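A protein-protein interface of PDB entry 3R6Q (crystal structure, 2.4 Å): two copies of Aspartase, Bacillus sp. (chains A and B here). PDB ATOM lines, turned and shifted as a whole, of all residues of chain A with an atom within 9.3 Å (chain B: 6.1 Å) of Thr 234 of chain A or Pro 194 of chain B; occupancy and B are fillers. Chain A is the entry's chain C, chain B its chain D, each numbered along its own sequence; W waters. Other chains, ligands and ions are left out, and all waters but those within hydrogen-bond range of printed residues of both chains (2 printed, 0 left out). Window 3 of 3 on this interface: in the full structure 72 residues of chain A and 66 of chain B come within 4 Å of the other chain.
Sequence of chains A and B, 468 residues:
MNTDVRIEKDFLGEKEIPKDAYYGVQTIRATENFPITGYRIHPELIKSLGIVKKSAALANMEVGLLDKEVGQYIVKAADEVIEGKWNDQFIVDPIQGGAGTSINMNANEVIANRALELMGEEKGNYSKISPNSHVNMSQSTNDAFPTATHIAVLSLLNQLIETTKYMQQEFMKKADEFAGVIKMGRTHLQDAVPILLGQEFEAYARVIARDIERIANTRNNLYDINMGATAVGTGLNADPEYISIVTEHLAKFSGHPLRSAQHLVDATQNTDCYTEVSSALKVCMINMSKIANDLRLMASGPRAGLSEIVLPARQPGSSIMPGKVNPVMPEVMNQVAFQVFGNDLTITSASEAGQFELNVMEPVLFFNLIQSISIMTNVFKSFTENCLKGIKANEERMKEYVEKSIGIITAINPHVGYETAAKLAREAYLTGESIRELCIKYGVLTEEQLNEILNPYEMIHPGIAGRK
No position is printed for both chains.
Of the 18 pairs that touch across the chains among the printed residues, none has its exchanged pair printed and touching as well.
Among the printed residues, pairs that only touch across the chains: Gly 235 of chain A with Pro 462 of chain B (3.2 Å), Glu 357 of chain A with Gly 185 of chain B (3.3 Å), Leu 236 of chain A with Met 459 of chain B (3.4 Å), Thr 234 of chain A with Pro 462 of chain B (3.4 Å), His 263 of chain A with Gln 199 of chain B (3.4 Å), Thr 234 of chain A with His 461 of chain B (3.4 Å), Val 232 of chain A with Ile 195 of chain B (3.5 Å), Glu 357 of chain A with Ile 195 of chain B (3.6 Å), Thr 234 of chain A with Pro 194 of chain B (3.6 Å), Val 232 of chain A with Val 193 of chain B (3.7 Å), Val 265 of chain A with Gln 199 of chain B (3.7 Å), Val 265 of chain A with Ile 195 of chain B (3.8 Å), Thr 234 of chain A with Ile 195 of chain B (3.9 Å), Thr 234 of chain A with Gln 199 of chain B (3.9 Å), Leu 236 of chain A with Ala 411 of chain B (3.9 Å) and Leu 236 of chain A with Thr 410 of chain B (3.99 Å).
Thr 234 of chain A touches just these residues of chain B: Pro 194 (3.6 Å), Ile 195 (3.9 Å), Gln 199 (3.9 Å), Ile 460 (3.2 Å), His 461 (3.4 Å) and Pro 462 (3.4 Å).
Val 193 of chain B touches just one residue of chain A: Val 232 (3.7 Å).
Printed residues of chain B within 4 Å of Asn 237 of chain A: Thr 410.
Printed residues of chain B within 4 Å of Gly 235 of chain A: Pro 462.
Printed residues of chain B within 4 Å of Leu 236 of chain A: Thr 410 (3.99 Å), Ala 411 (3.9 Å) and Met 459 (3.4 Å).
Asp 239 of chain A touches none of the printed residues of chain B.
The nearest printed residue of chain A that does not touch Pro 194 of chain B is Leu 236 of chain A (4.9 Å).
The backbone NH of Leu 196 of chain B lies within hydrogen-bond range of the side-chain amide oxygen of Gln 199 of chain B (3.1 Å).
The backbone carbonyl oxygen (O) of Gly 407 of chain B is in hydrogen-bond range of the side-chain hydroxyl (OG1) of Thr 410 of chain B (3.2 Å).
Of the 22 printed residues of chain A, 8 touch a printed residue of chain B.
Printed residues of chain A that touch a printed residue of chain B: Val 232, Thr 234, Gly 235, Leu 236, Asn 237, His 263, Val 265 and Glu 357.
Hydrophobic or aromatic side chains of chain A that line the printed part of chain B: Val 232, Leu 236, His 263 and Val 265.
Hydrophobic or aromatic side chains of chain B within 4 Å of the printed part of chain A: Val 193, Ile 195 and Pro 462.
Along chain B the printed residues that touch a printed residue of chain A span positions 185 to 462.
Among the printed residues, 18 pairs touch across the chains.
Water W2 bridges the side-chain amide oxygen (OD1) of Asn 237 of chain A (2.7 Å) and the backbone carbonyl oxygen (O) of Ala 411 of chain B (2.8 Å).
The backbone carbonyl oxygen (O) of Thr 410 of chain B is in hydrogen-bond range of the side-chain amide nitrogen (ND2) of Asn 237 of chain A, 2.7 Å away.
The backbone carbonyl oxygen of Ile 460 of chain B sits close to the backbone carbonyl oxygen of Thr 234 of chain A, 3.2 Å away.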
ATOM      1  N   ASN A 226       2.164  16.726 -17.262  1.00  0.00           N
ATOM      2  CA  ASN A 226       1.924  18.142 -16.926  1.00  0.00           C
ATOM      3  C   ASN A 226       2.499  18.596 -15.587  1.00  0.00           C
ATOM      4  O   ASN A 226       2.074  19.599 -15.015  1.00  0.00           O
ATOM      5  CB  ASN A 226       0.425  18.482 -17.015  1.00  0.00           C
ATOM      6  CG  ASN A 226      -0.394  17.868 -15.881  1.00  0.00           C
ATOM      7  OD1 ASN A 226       0.001  16.870 -15.257  1.00  0.00           O
ATOM      8  ND2 ASN A 226      -1.537  18.472 -15.605  1.00  0.00           N
ATOM      9  N   GLY A 228       4.098  20.386 -12.787  1.00  0.00           N
ATOM     10  CA  GLY A 228       4.396  21.822 -12.680  1.00  0.00           C
ATOM     11  C   GLY A 228       3.313  22.731 -13.253  1.00  0.00           C
ATOM     12  O   GLY A 228       3.509  23.941 -13.418  1.00  0.00           O
ATOM     13  N   ALA A 229       2.165  22.143 -13.565  1.00  0.00           N
ATOM     14  CA  ALA A 229       1.043  22.878 -14.139  1.00  0.00           C
ATOM     15  C   ALA A 229       0.477  23.886 -13.148  1.00  0.00           C
ATOM     16  O   ALA A 229      -0.057  24.914 -13.558  1.00  0.00           O
ATOM     17  CB  ALA A 229      -0.059  21.895 -14.582  1.00  0.00           C
ATOM     18  N   THR A 230       0.661  23.593 -11.853  1.00  0.00           N
ATOM     19  CA  THR A 230      -0.126  24.150 -10.744  1.00  0.00           C
ATOM     20  C   THR A 230      -1.613  24.006 -11.058  1.00  0.00           C
ATOM     21  O   THR A 230      -1.977  23.211 -11.933  1.00  0.00           O
ATOM     22  CB  THR A 230       0.293  25.592 -10.292  1.00  0.00           C
ATOM     23  OG1 THR A 230       0.127  26.527 -11.366  1.00  0.00           O
ATOM     24  CG2 THR A 230       1.760  25.616  -9.807  1.00  0.00           C
ATOM     25  N   ALA A 231      -2.466  24.753 -10.363  1.00  0.00           N
ATOM     26  CA  ALA A 231      -3.922  24.557 -10.431  1.00  0.00           C
ATOM     27  C   ALA A 231      -4.523  24.378 -11.837  1.00  0.00           C
ATOM     28  O   ALA A 231      -5.413  23.559 -12.032  1.00  0.00           O
ATOM     29  CB  ALA A 231      -4.644  25.690  -9.697  1.00  0.00           C
ATOM     30  N   VAL A 232      -4.028  25.137 -12.807  1.00  0.00           N
ATOM     31  CA  VAL A 232      -4.744  25.310 -14.061  1.00  0.00           C
ATOM     32  C   VAL A 232      -3.901  25.014 -15.309  1.00  0.00           C
ATOM     33  O   VAL A 232      -4.438  24.854 -16.421  1.00  0.00           O
ATOM     34  CB  VAL A 232      -5.345  26.735 -14.093  1.00  0.00           C
ATOM     35  CG1 VAL A 232      -5.257  27.363 -15.476  1.00  0.00           C
ATOM     36  CG2 VAL A 232      -6.769  26.728 -13.566  1.00  0.00           C
ATOM     37  N   GLY A 233      -2.584  24.943 -15.127  1.00  0.00           N
ATOM     38  CA  GLY A 233      -1.662  24.746 -16.249  1.00  0.00           C
ATOM     39  C   GLY A 233      -0.767  25.932 -16.559  1.00  0.00           C
ATOM     40  O   GLY A 233       0.196  25.803 -17.316  1.00  0.00           O
ATOM     41  N   THR A 234      -1.071  27.088 -15.971  1.00  0.00           N
ATOM     42  CA  THR A 234      -0.316  28.316 -16.239  1.00  0.00           C
ATOM     43  C   THR A 234       1.074  28.302 -15.600  1.00  0.00           C
ATOM     44  O   THR A 234       1.933  29.091 -15.969  1.00  0.00           O
ATOM     45  CB  THR A 234      -1.069  29.564 -15.766  1.00  0.00           C
ATOM     46  OG1 THR A 234      -1.309  29.469 -14.358  1.00  0.00           O
ATOM     47  CG2 THR A 234      -2.393  29.714 -16.509  1.00  0.00           C
ATOM     48  N   GLY A 235       1.282  27.404 -14.646  1.00  0.00           N
ATOM     49  CA  GLY A 235       2.571  27.242 -13.992  1.00  0.00           C
ATOM     50  C   GLY A 235       2.963  28.450 -13.169  1.00  0.00           C
ATOM     51  O   GLY A 235       4.152  28.762 -13.054  1.00  0.00           O
ATOM     52  N   LEU A 236       1.955  29.130 -12.615  1.00  0.00           N
ATOM     53  CA  LEU A 236       2.146  30.295 -11.759  1.00  0.00           C
ATOM     54  C   LEU A 236       2.831  29.926 -10.445  1.00  0.00           C
ATOM     55  O   LEU A 236       2.356  29.041  -9.723  1.00  0.00           O
ATOM     56  CB  LEU A 236       0.803  30.964 -11.476  1.00  0.00           C
ATOM     57  CG  LEU A 236       0.826  32.164 -10.521  1.00  0.00           C
ATOM     58  CD1 LEU A 236       1.622  33.339 -11.104  1.00  0.00           C
ATOM     59  CD2 LEU A 236      -0.594  32.586 -10.202  1.00  0.00           C
ATOM     60  N   ASN A 237       3.936  30.616 -10.153  1.00  0.00           N
ATOM     61  CA  ASN A 237       4.825  30.352  -8.997  1.00  0.00           C
ATOM     62  C   ASN A 237       5.618  29.049  -9.060  1.00  0.00           C
ATOM     63  O   ASN A 237       6.383  28.749  -8.145  1.00  0.00           O
ATOM     64  CB  ASN A 237       4.093  30.452  -7.649  1.00  0.00           C
ATOM     65  CG  ASN A 237       3.418  31.795  -7.441  1.00  0.00           C
ATOM     66  OD1 ASN A 237       3.955  32.853  -7.797  1.00  0.00           O
ATOM     67  ND2 ASN A 237       2.228  31.759  -6.853  1.00  0.00           N
ATOM     68  N   ALA A 238       5.438  28.279 -10.133  1.00  0.00           N
ATOM     69  CA  ALA A 238       6.238  27.073 -10.356  1.00  0.00           C
ATOM     70  C   ALA A 238       7.660  27.456 -10.771  1.00  0.00           C
ATOM     71  O   ALA A 238       7.867  28.487 -11.409  1.00  0.00           O
ATOM     72  CB  ALA A 238       5.587  26.176 -11.414  1.00  0.00           C
ATOM     73  N   ASP A 239       8.630  26.625 -10.390  1.00  0.00           N
ATOM     74  CA  ASP A 239      10.045  26.845 -10.702  1.00  0.00           C
ATOM     75  C   ASP A 239      10.445  26.054 -11.951  1.00  0.00           C
ATOM     76  O   ASP A 239      10.354  24.828 -11.952  1.00  0.00           O
ATOM     77  CB  ASP A 239      10.891  26.410  -9.507  1.00  0.00           C
ATOM     78  CG  ASP A 239      12.365  26.757  -9.653  1.00  0.00           C
ATOM     79  OD1 ASP A 239      13.099  26.560  -8.665  1.00  0.00           O
ATOM     80  OD2 ASP A 239      12.805  27.222 -10.727  1.00  0.00           O
ATOM     81  N   ILE A 243      10.700  21.889 -12.484  1.00  0.00           N
ATOM     82  CA  ILE A 243       9.969  21.253 -13.567  1.00  0.00           C
ATOM     83  C   ILE A 243      10.867  20.304 -14.362  1.00  0.00           C
ATOM     84  O   ILE A 243      10.521  19.136 -14.535  1.00  0.00           O
ATOM     85  CB  ILE A 243       9.256  22.307 -14.460  1.00  0.00           C
ATOM     86  CG1 ILE A 243       7.936  22.732 -13.801  1.00  0.00           C
ATOM     87  CG2 ILE A 243       8.991  21.768 -15.868  1.00  0.00           C
ATOM     88  CD1 ILE A 243       7.399  24.093 -14.243  1.00  0.00           C
ATOM     89  N   HIS A 263       2.527  22.566 -23.899  1.00  0.00           N
ATOM     90  CA  HIS A 263       1.512  23.508 -23.461  1.00  0.00           C
ATOM     91  C   HIS A 263       0.800  22.874 -22.281  1.00  0.00           C
ATOM     92  O   HIS A 263      -0.004  21.945 -22.460  1.00  0.00           O
ATOM     93  CB  HIS A 263       0.542  23.779 -24.605  1.00  0.00           C
ATOM     94  CG  HIS A 263      -0.272  25.024 -24.446  1.00  0.00           C
ATOM     95  ND1 HIS A 263      -1.538  25.019 -23.906  1.00  0.00           N
ATOM     96  CD2 HIS A 263      -0.020  26.305 -24.801  1.00  0.00           C
ATOM     97  CE1 HIS A 263      -2.022  26.250 -23.908  1.00  0.00           C
ATOM     98  NE2 HIS A 263      -1.122  27.050 -24.448  1.00  0.00           N
ATOM     99  N   LEU A 264       1.100  23.370 -21.079  1.00  0.00           N
ATOM    100  CA  LEU A 264       0.624  22.740 -19.846  1.00  0.00           C
ATOM    101  C   LEU A 264      -0.836  23.053 -19.517  1.00  0.00           C
ATOM    102  O   LEU A 264      -1.482  22.302 -18.786  1.00  0.00           O
ATOM    103  CB  LEU A 264       1.562  23.027 -18.666  1.00  0.00           C
ATOM    104  CG  LEU A 264       3.036  22.594 -18.821  1.00  0.00           C
ATOM    105  CD1 LEU A 264       3.877  23.004 -17.621  1.00  0.00           C
ATOM    106  CD2 LEU A 264       3.196  21.092 -19.093  1.00  0.00           C
ATOM    107  N   VAL A 265      -1.361  24.144 -20.073  1.00  0.00           N
ATOM    108  CA  VAL A 265      -2.803  24.411 -20.004  1.00  0.00           C
ATOM    109  C   VAL A 265      -3.560  23.315 -20.774  1.00  0.00           C
ATOM    110  O   VAL A 265      -4.493  22.695 -20.242  1.00  0.00           O
ATOM    111  CB  VAL A 265      -3.177  25.839 -20.494  1.00  0.00           C
ATOM    112  CG1 VAL A 265      -4.657  25.932 -20.827  1.00  0.00           C
ATOM    113  CG2 VAL A 265      -2.817  26.884 -19.430  1.00  0.00           C
ATOM    114  N   ASP A 266      -3.118  23.064 -22.004  1.00  0.00           N
ATOM    115  CA  ASP A 266      -3.635  21.962 -22.819  1.00  0.00           C
ATOM    116  C   ASP A 266      -3.524  20.616 -22.109  1.00  0.00           C
ATOM    117  O   ASP A 266      -4.450  19.815 -22.162  1.00  0.00           O
ATOM    118  CB  ASP A 266      -2.923  21.912 -24.182  1.00  0.00           C
ATOM    119  CG  ASP A 266      -3.124  20.595 -24.911  1.00  0.00           C
ATOM    120  OD1 ASP A 266      -4.246  20.025 -24.876  1.00  0.00           O
ATOM    121  OD2 ASP A 266      -2.152  20.124 -25.543  1.00  0.00           O
ATOM    122  N   ALA A 267      -2.400  20.368 -21.445  1.00  0.00           N
ATOM    123  CA  ALA A 267      -2.180  19.056 -20.846  1.00  0.00           C
ATOM    124  C   ALA A 267      -3.022  18.855 -19.585  1.00  0.00           C
ATOM    125  O   ALA A 267      -3.317  17.728 -19.217  1.00  0.00           O
ATOM    126  CB  ALA A 267      -0.724  18.843 -20.550  1.00  0.00           C
ATOM    127  N   THR A 268      -3.410  19.952 -18.944  1.00  0.00           N
ATOM    128  CA  THR A 268      -4.174  19.890 -17.708  1.00  0.00           C
ATOM    129  C   THR A 268      -5.670  19.679 -17.960  1.00  0.00           C
ATOM    130  O   THR A 268      -6.342  19.052 -17.140  1.00  0.00           O
ATOM    131  CB  THR A 268      -3.971  21.165 -16.831  1.00  0.00           C
ATOM    132  OG1 THR A 268      -2.575  21.392 -16.617  1.00  0.00           O
ATOM    133  CG2 THR A 268      -4.656  21.017 -15.477  1.00  0.00           C
ATOM    134  N   GLN A 269      -6.195  20.200 -19.073  1.00  0.00           N
ATOM    135  CA  GLN A 269      -7.650  20.214 -19.280  1.00  0.00           C
ATOM    136  C   GLN A 269      -8.186  19.186 -20.278  1.00  0.00           C
ATOM    137  O   GLN A 269      -9.377  18.836 -20.236  1.00  0.00           O
ATOM    138  CB  GLN A 269      -8.150  21.614 -19.623  1.00  0.00           C
ATOM    139  CG  GLN A 269      -7.659  22.181 -20.932  1.00  0.00           C
ATOM    140  CD  GLN A 269      -8.257  23.548 -21.200  1.00  0.00           C
ATOM    141  OE1 GLN A 269      -9.059  23.719 -22.123  1.00  0.00           O
ATOM    142  NE2 GLN A 269      -7.888  24.533 -20.372  1.00  0.00           N
ATOM    143  N   GLU A 357     -10.952  24.493 -17.296  1.00  0.00           N
ATOM    144  CA  GLU A 357      -9.565  24.148 -17.047  1.00  0.00           C
ATOM    145  C   GLU A 357      -9.348  22.752 -16.449  1.00  0.00           C
ATOM    146  O   GLU A 357      -8.205  22.368 -16.252  1.00  0.00           O
ATOM    147  CB  GLU A 357      -8.898  25.220 -16.173  1.00  0.00           C
ATOM    148  CG  GLU A 357      -8.482  26.452 -16.958  1.00  0.00           C
ATOM    149  CD  GLU A 357      -9.641  27.077 -17.726  1.00  0.00           C
ATOM    150  OE1 GLU A 357      -9.678  26.953 -18.970  1.00  0.00           O
ATOM    151  OE2 GLU A 357     -10.533  27.661 -17.081  1.00  0.00           O
ATOM    152  N   ILE B 182      -7.096  38.545 -20.554  1.00  0.00           N
ATOM    153  CA  ILE B 182      -7.023  37.947 -19.225  1.00  0.00           C
ATOM    154  C   ILE B 182      -8.422  37.597 -18.680  1.00  0.00           C
ATOM    155  O   ILE B 182      -9.374  38.369 -18.831  1.00  0.00           O
ATOM    156  CB  ILE B 182      -6.255  38.880 -18.243  1.00  0.00           C
ATOM    157  CG1 ILE B 182      -5.930  38.166 -16.921  1.00  0.00           C
ATOM    158  CG2 ILE B 182      -7.033  40.157 -17.962  1.00  0.00           C
ATOM    159  CD1 ILE B 182      -4.843  37.118 -17.028  1.00  0.00           C
ATOM    160  N   LYS B 183      -8.546  36.418 -18.085  1.00  0.00           N
ATOM    161  CA  LYS B 183      -9.822  35.961 -17.520  1.00  0.00           C
ATOM    162  C   LYS B 183      -9.557  35.070 -16.299  1.00  0.00           C
ATOM    163  O   LYS B 183      -8.399  34.795 -15.944  1.00  0.00           O
ATOM    164  CB  LYS B 183     -10.706  35.219 -18.561  1.00  0.00           C
ATOM    165  CG  LYS B 183     -10.064  33.951 -19.154  1.00  0.00           C
ATOM    166  CD  LYS B 183     -11.034  33.046 -19.918  1.00  0.00           C
ATOM    167  CE  LYS B 183     -11.624  31.976 -19.007  1.00  0.00           C
ATOM    168  NZ  LYS B 183     -12.571  31.084 -19.718  1.00  0.00           N
ATOM    169  N   MET B 184     -10.638  34.639 -15.659  1.00  0.00           N
ATOM    170  CA  MET B 184     -10.557  33.745 -14.519  1.00  0.00           C
ATOM    171  C   MET B 184     -10.688  32.277 -14.956  1.00  0.00           C
ATOM    172  O   MET B 184     -11.687  31.878 -15.573  1.00  0.00           O
ATOM    173  CB  MET B 184     -11.626  34.123 -13.503  1.00  0.00           C
ATOM    174  CG  MET B 184     -11.167  34.010 -12.081  1.00  0.00           C
ATOM    175  SD  MET B 184      -9.701  35.016 -11.767  1.00  0.00           S
ATOM    176  CE  MET B 184      -8.905  34.024 -10.507  1.00  0.00           C
ATOM    177  N   GLY B 185      -9.661  31.483 -14.683  1.00  0.00           N
ATOM    178  CA  GLY B 185      -9.741  30.046 -14.905  1.00  0.00           C
ATOM    179  C   GLY B 185     -10.655  29.354 -13.900  1.00  0.00           C
ATOM    180  O   GLY B 185     -10.804  29.800 -12.757  1.00  0.00           O
ATOM    181  N   ALA B 192     -10.710  29.776  -9.963  1.00  0.00           N
ATOM    182  CA  ALA B 192      -9.425  29.241  -9.558  1.00  0.00           C
ATOM    183  C   ALA B 192      -8.339  30.311  -9.681  1.00  0.00           C
ATOM    184  O   ALA B 192      -8.230  31.159  -8.808  1.00  0.00           O
ATOM    185  CB  ALA B 192      -9.088  27.994 -10.378  1.00  0.00           C
ATOM    186  N   VAL B 193      -7.565  30.285 -10.769  1.00  0.00           N
ATOM    187  CA  VAL B 193      -6.479  31.254 -10.985  1.00  0.00           C
ATOM    188  C   VAL B 193      -6.528  31.899 -12.402  1.00  0.00           C
ATOM    189  O   VAL B 193      -7.178  31.370 -13.308  1.00  0.00           O
ATOM    190  CB  VAL B 193      -5.075  30.622 -10.705  1.00  0.00           C
ATOM    191  CG1 VAL B 193      -4.922  30.208  -9.223  1.00  0.00           C
ATOM    192  CG2 VAL B 193      -4.830  29.445 -11.627  1.00  0.00           C
ATOM    193  N   PRO B 194      -5.856  33.055 -12.588  1.00  0.00           N
ATOM    194  CA  PRO B 194      -5.971  33.741 -13.869  1.00  0.00           C
ATOM    195  C   PRO B 194      -5.458  32.908 -15.037  1.00  0.00           C
ATOM    196  O   PRO B 194      -4.486  32.172 -14.905  1.00  0.00           O
ATOM    197  CB  PRO B 194      -5.112  34.997 -13.660  1.00  0.00           C
ATOM    198  CG  PRO B 194      -5.176  35.233 -12.178  1.00  0.00           C
ATOM    199  CD  PRO B 194      -5.110  33.868 -11.605  1.00  0.00           C
ATOM    200  N   ILE B 195      -6.157  32.995 -16.157  1.00  0.00           N
ATOM    201  CA  ILE B 195      -5.741  32.343 -17.379  1.00  0.00           C
ATOM    202  C   ILE B 195      -6.009  33.320 -18.522  1.00  0.00           C
ATOM    203  O   ILE B 195      -6.816  34.241 -18.373  1.00  0.00           O
ATOM    204  CB  ILE B 195      -6.449  30.955 -17.575  1.00  0.00           C
ATOM    205  CG1 ILE B 195      -5.655  30.068 -18.534  1.00  0.00           C
ATOM    206  CG2 ILE B 195      -7.913  31.104 -18.023  1.00  0.00           C
ATOM    207  CD1 ILE B 195      -6.128  28.633 -18.590  1.00  0.00           C
ATOM    208  N   LEU B 196      -5.313  33.147 -19.637  1.00  0.00           N
ATOM    209  CA  LEU B 196      -5.569  33.956 -20.817  1.00  0.00           C
ATOM    210  C   LEU B 196      -6.593  33.248 -21.674  1.00  0.00           C
ATOM    211  O   LEU B 196      -6.553  32.034 -21.794  1.00  0.00           O
ATOM    212  CB  LEU B 196      -4.292  34.151 -21.621  1.00  0.00           C
ATOM    213  CG  LEU B 196      -3.149  34.912 -20.944  1.00  0.00           C
ATOM    214  CD1 LEU B 196      -1.891  34.853 -21.815  1.00  0.00           C
ATOM    215  CD2 LEU B 196      -3.502  36.375 -20.604  1.00  0.00           C
ATOM    216  N   GLN B 199      -4.948  31.089 -24.143  1.00  0.00           N
ATOM    217  CA  GLN B 199      -4.417  29.826 -23.660  1.00  0.00           C
ATOM    218  C   GLN B 199      -5.477  28.718 -23.766  1.00  0.00           C
ATOM    219  O   GLN B 199      -5.160  27.576 -24.115  1.00  0.00           O
ATOM    220  CB  GLN B 199      -3.884  29.969 -22.228  1.00  0.00           C
ATOM    221  CG  GLN B 199      -2.475  30.576 -22.141  1.00  0.00           C
ATOM    222  CD  GLN B 199      -2.035  30.855 -20.710  1.00  0.00           C
ATOM    223  OE1 GLN B 199      -2.758  31.492 -19.932  1.00  0.00           O
ATOM    224  NE2 GLN B 199      -0.847  30.373 -20.351  1.00  0.00           N
ATOM    225  N   VAL B 402     -11.250  39.063 -12.826  1.00  0.00           N
ATOM    226  CA  VAL B 402      -9.902  38.874 -12.321  1.00  0.00           C
ATOM    227  C   VAL B 402      -9.580  39.879 -11.222  1.00  0.00           C
ATOM    228  O   VAL B 402      -9.074  39.474 -10.181  1.00  0.00           O
ATOM    229  CB  VAL B 402      -8.846  38.867 -13.458  1.00  0.00           C
ATOM    230  CG1 VAL B 402      -7.418  38.809 -12.912  1.00  0.00           C
ATOM    231  CG2 VAL B 402      -9.094  37.688 -14.391  1.00  0.00           C
ATOM    232  N   SER B 405     -11.570  38.867  -7.986  1.00  0.00           N
ATOM    233  CA  SER B 405     -11.455  37.486  -7.518  1.00  0.00           C
ATOM    234  C   SER B 405     -10.566  37.322  -6.275  1.00  0.00           C
ATOM    235  O   SER B 405      -9.824  38.228  -5.881  1.00  0.00           O
ATOM    236  CB  SER B 405     -10.931  36.583  -8.644  1.00  0.00           C
ATOM    237  OG  SER B 405      -9.531  36.740  -8.824  1.00  0.00           O
ATOM    238  N   GLY B 407      -8.643  34.357  -6.178  1.00  0.00           N
ATOM    239  CA  GLY B 407      -7.536  33.600  -6.760  1.00  0.00           C
ATOM    240  C   GLY B 407      -6.365  34.428  -7.244  1.00  0.00           C
ATOM    241  O   GLY B 407      -5.268  33.912  -7.412  1.00  0.00           O
ATOM    242  N   ILE B 408      -6.596  35.716  -7.476  1.00  0.00           N
ATOM    243  CA  ILE B 408      -5.514  36.646  -7.770  1.00  0.00           C
ATOM    244  C   ILE B 408      -4.496  36.747  -6.603  1.00  0.00           C
ATOM    245  O   ILE B 408      -3.367  37.212  -6.794  1.00  0.00           O
ATOM    246  CB  ILE B 408      -6.073  38.041  -8.187  1.00  0.00           C
ATOM    247  CG1 ILE B 408      -5.136  38.732  -9.172  1.00  0.00           C
ATOM    248  CG2 ILE B 408      -6.390  38.928  -6.968  1.00  0.00           C
ATOM    249  CD1 ILE B 408      -5.764  39.922  -9.872  1.00  0.00           C
ATOM    250  N   THR B 410      -2.973  34.292  -5.336  1.00  0.00           N
ATOM    251  CA  THR B 410      -1.937  33.311  -5.645  1.00  0.00           C
ATOM    252  C   THR B 410      -0.709  33.967  -6.286  1.00  0.00           C
ATOM    253  O   THR B 410       0.424  33.566  -6.017  1.00  0.00           O
ATOM    254  CB  THR B 410      -2.505  32.133  -6.490  1.00  0.00           C
ATOM    255  OG1 THR B 410      -3.665  31.605  -5.831  1.00  0.00           O
ATOM    256  CG2 THR B 410      -1.480  31.005  -6.647  1.00  0.00           C
ATOM    257  N   ALA B 411      -0.938  34.993  -7.100  1.00  0.00           N
ATOM    258  CA  ALA B 411       0.152  35.789  -7.664  1.00  0.00           C
ATOM    259  C   ALA B 411       0.886  36.616  -6.600  1.00  0.00           C
ATOM    260  O   ALA B 411       2.096  36.806  -6.681  1.00  0.00           O
ATOM    261  CB  ALA B 411      -0.372  36.701  -8.776  1.00  0.00           C
ATOM    262  N   MET B 459       1.260  36.653 -14.672  1.00  0.00           N
ATOM    263  CA  MET B 459       0.321  35.848 -13.912  1.00  0.00           C
ATOM    264  C   MET B 459       0.055  34.479 -14.531  1.00  0.00           C
ATOM    265  O   MET B 459      -0.362  33.556 -13.839  1.00  0.00           O
ATOM    266  CB  MET B 459      -0.998  36.586 -13.764  1.00  0.00           C
ATOM    267  CG  MET B 459      -0.948  37.752 -12.825  1.00  0.00           C
ATOM    268  SD  MET B 459      -2.593  38.177 -12.226  1.00  0.00           S
ATOM    269  CE  MET B 459      -3.374  38.837 -13.705  1.00  0.00           C
ATOM    270  N   ILE B 460       0.317  34.342 -15.825  1.00  0.00           N
ATOM    271  CA  ILE B 460      -0.091  33.136 -16.537  1.00  0.00           C
ATOM    272  C   ILE B 460       1.057  32.302 -17.127  1.00  0.00           C
ATOM    273  O   ILE B 460       0.824  31.393 -17.919  1.00  0.00           O
ATOM    274  CB  ILE B 460      -1.153  33.470 -17.596  1.00  0.00           C
ATOM    275  CG1 ILE B 460      -0.637  34.546 -18.530  1.00  0.00           C
ATOM    276  CG2 ILE B 460      -2.411  33.974 -16.939  1.00  0.00           C
ATOM    277  CD1 ILE B 460       0.230  34.030 -19.630  1.00  0.00           C
ATOM    278  N   HIS B 461       2.286  32.614 -16.736  1.00  0.00           N
ATOM    279  CA  HIS B 461       3.468  31.897 -17.216  1.00  0.00           C
ATOM    280  C   HIS B 461       4.438  31.557 -16.084  1.00  0.00           C
ATOM    281  O   HIS B 461       4.525  32.303 -15.104  1.00  0.00           O
ATOM    282  CB  HIS B 461       4.180  32.709 -18.307  1.00  0.00           C
ATOM    283  CG  HIS B 461       3.682  32.423 -19.690  1.00  0.00           C
ATOM    284  ND1 HIS B 461       2.724  33.194 -20.313  1.00  0.00           N
ATOM    285  CD2 HIS B 461       3.994  31.435 -20.563  1.00  0.00           C
ATOM    286  CE1 HIS B 461       2.472  32.699 -21.513  1.00  0.00           C
ATOM    287  NE2 HIS B 461       3.229  31.630 -21.688  1.00  0.00           N
ATOM    288  N   PRO B 462       5.171  30.428 -16.211  1.00  0.00           N
ATOM    289  CA  PRO B 462       6.170  30.078 -15.201  1.00  0.00           C
ATOM    290  C   PRO B 462       7.082  31.261 -14.845  1.00  0.00           C
ATOM    291  O   PRO B 462       7.742  31.836 -15.718  1.00  0.00           O
ATOM    292  CB  PRO B 462       6.957  28.946 -15.866  1.00  0.00           C
ATOM    293  CG  PRO B 462       5.981  28.302 -16.771  1.00  0.00           C
ATOM    294  CD  PRO B 462       5.073  29.398 -17.261  1.00  0.00           C
HETATM  295  O   HOH W   1     -12.486  29.640 -17.151  1.00  0.00           O
HETATM  296  O   HOH W   2       3.779  35.441  -8.532  1.00  0.00           O
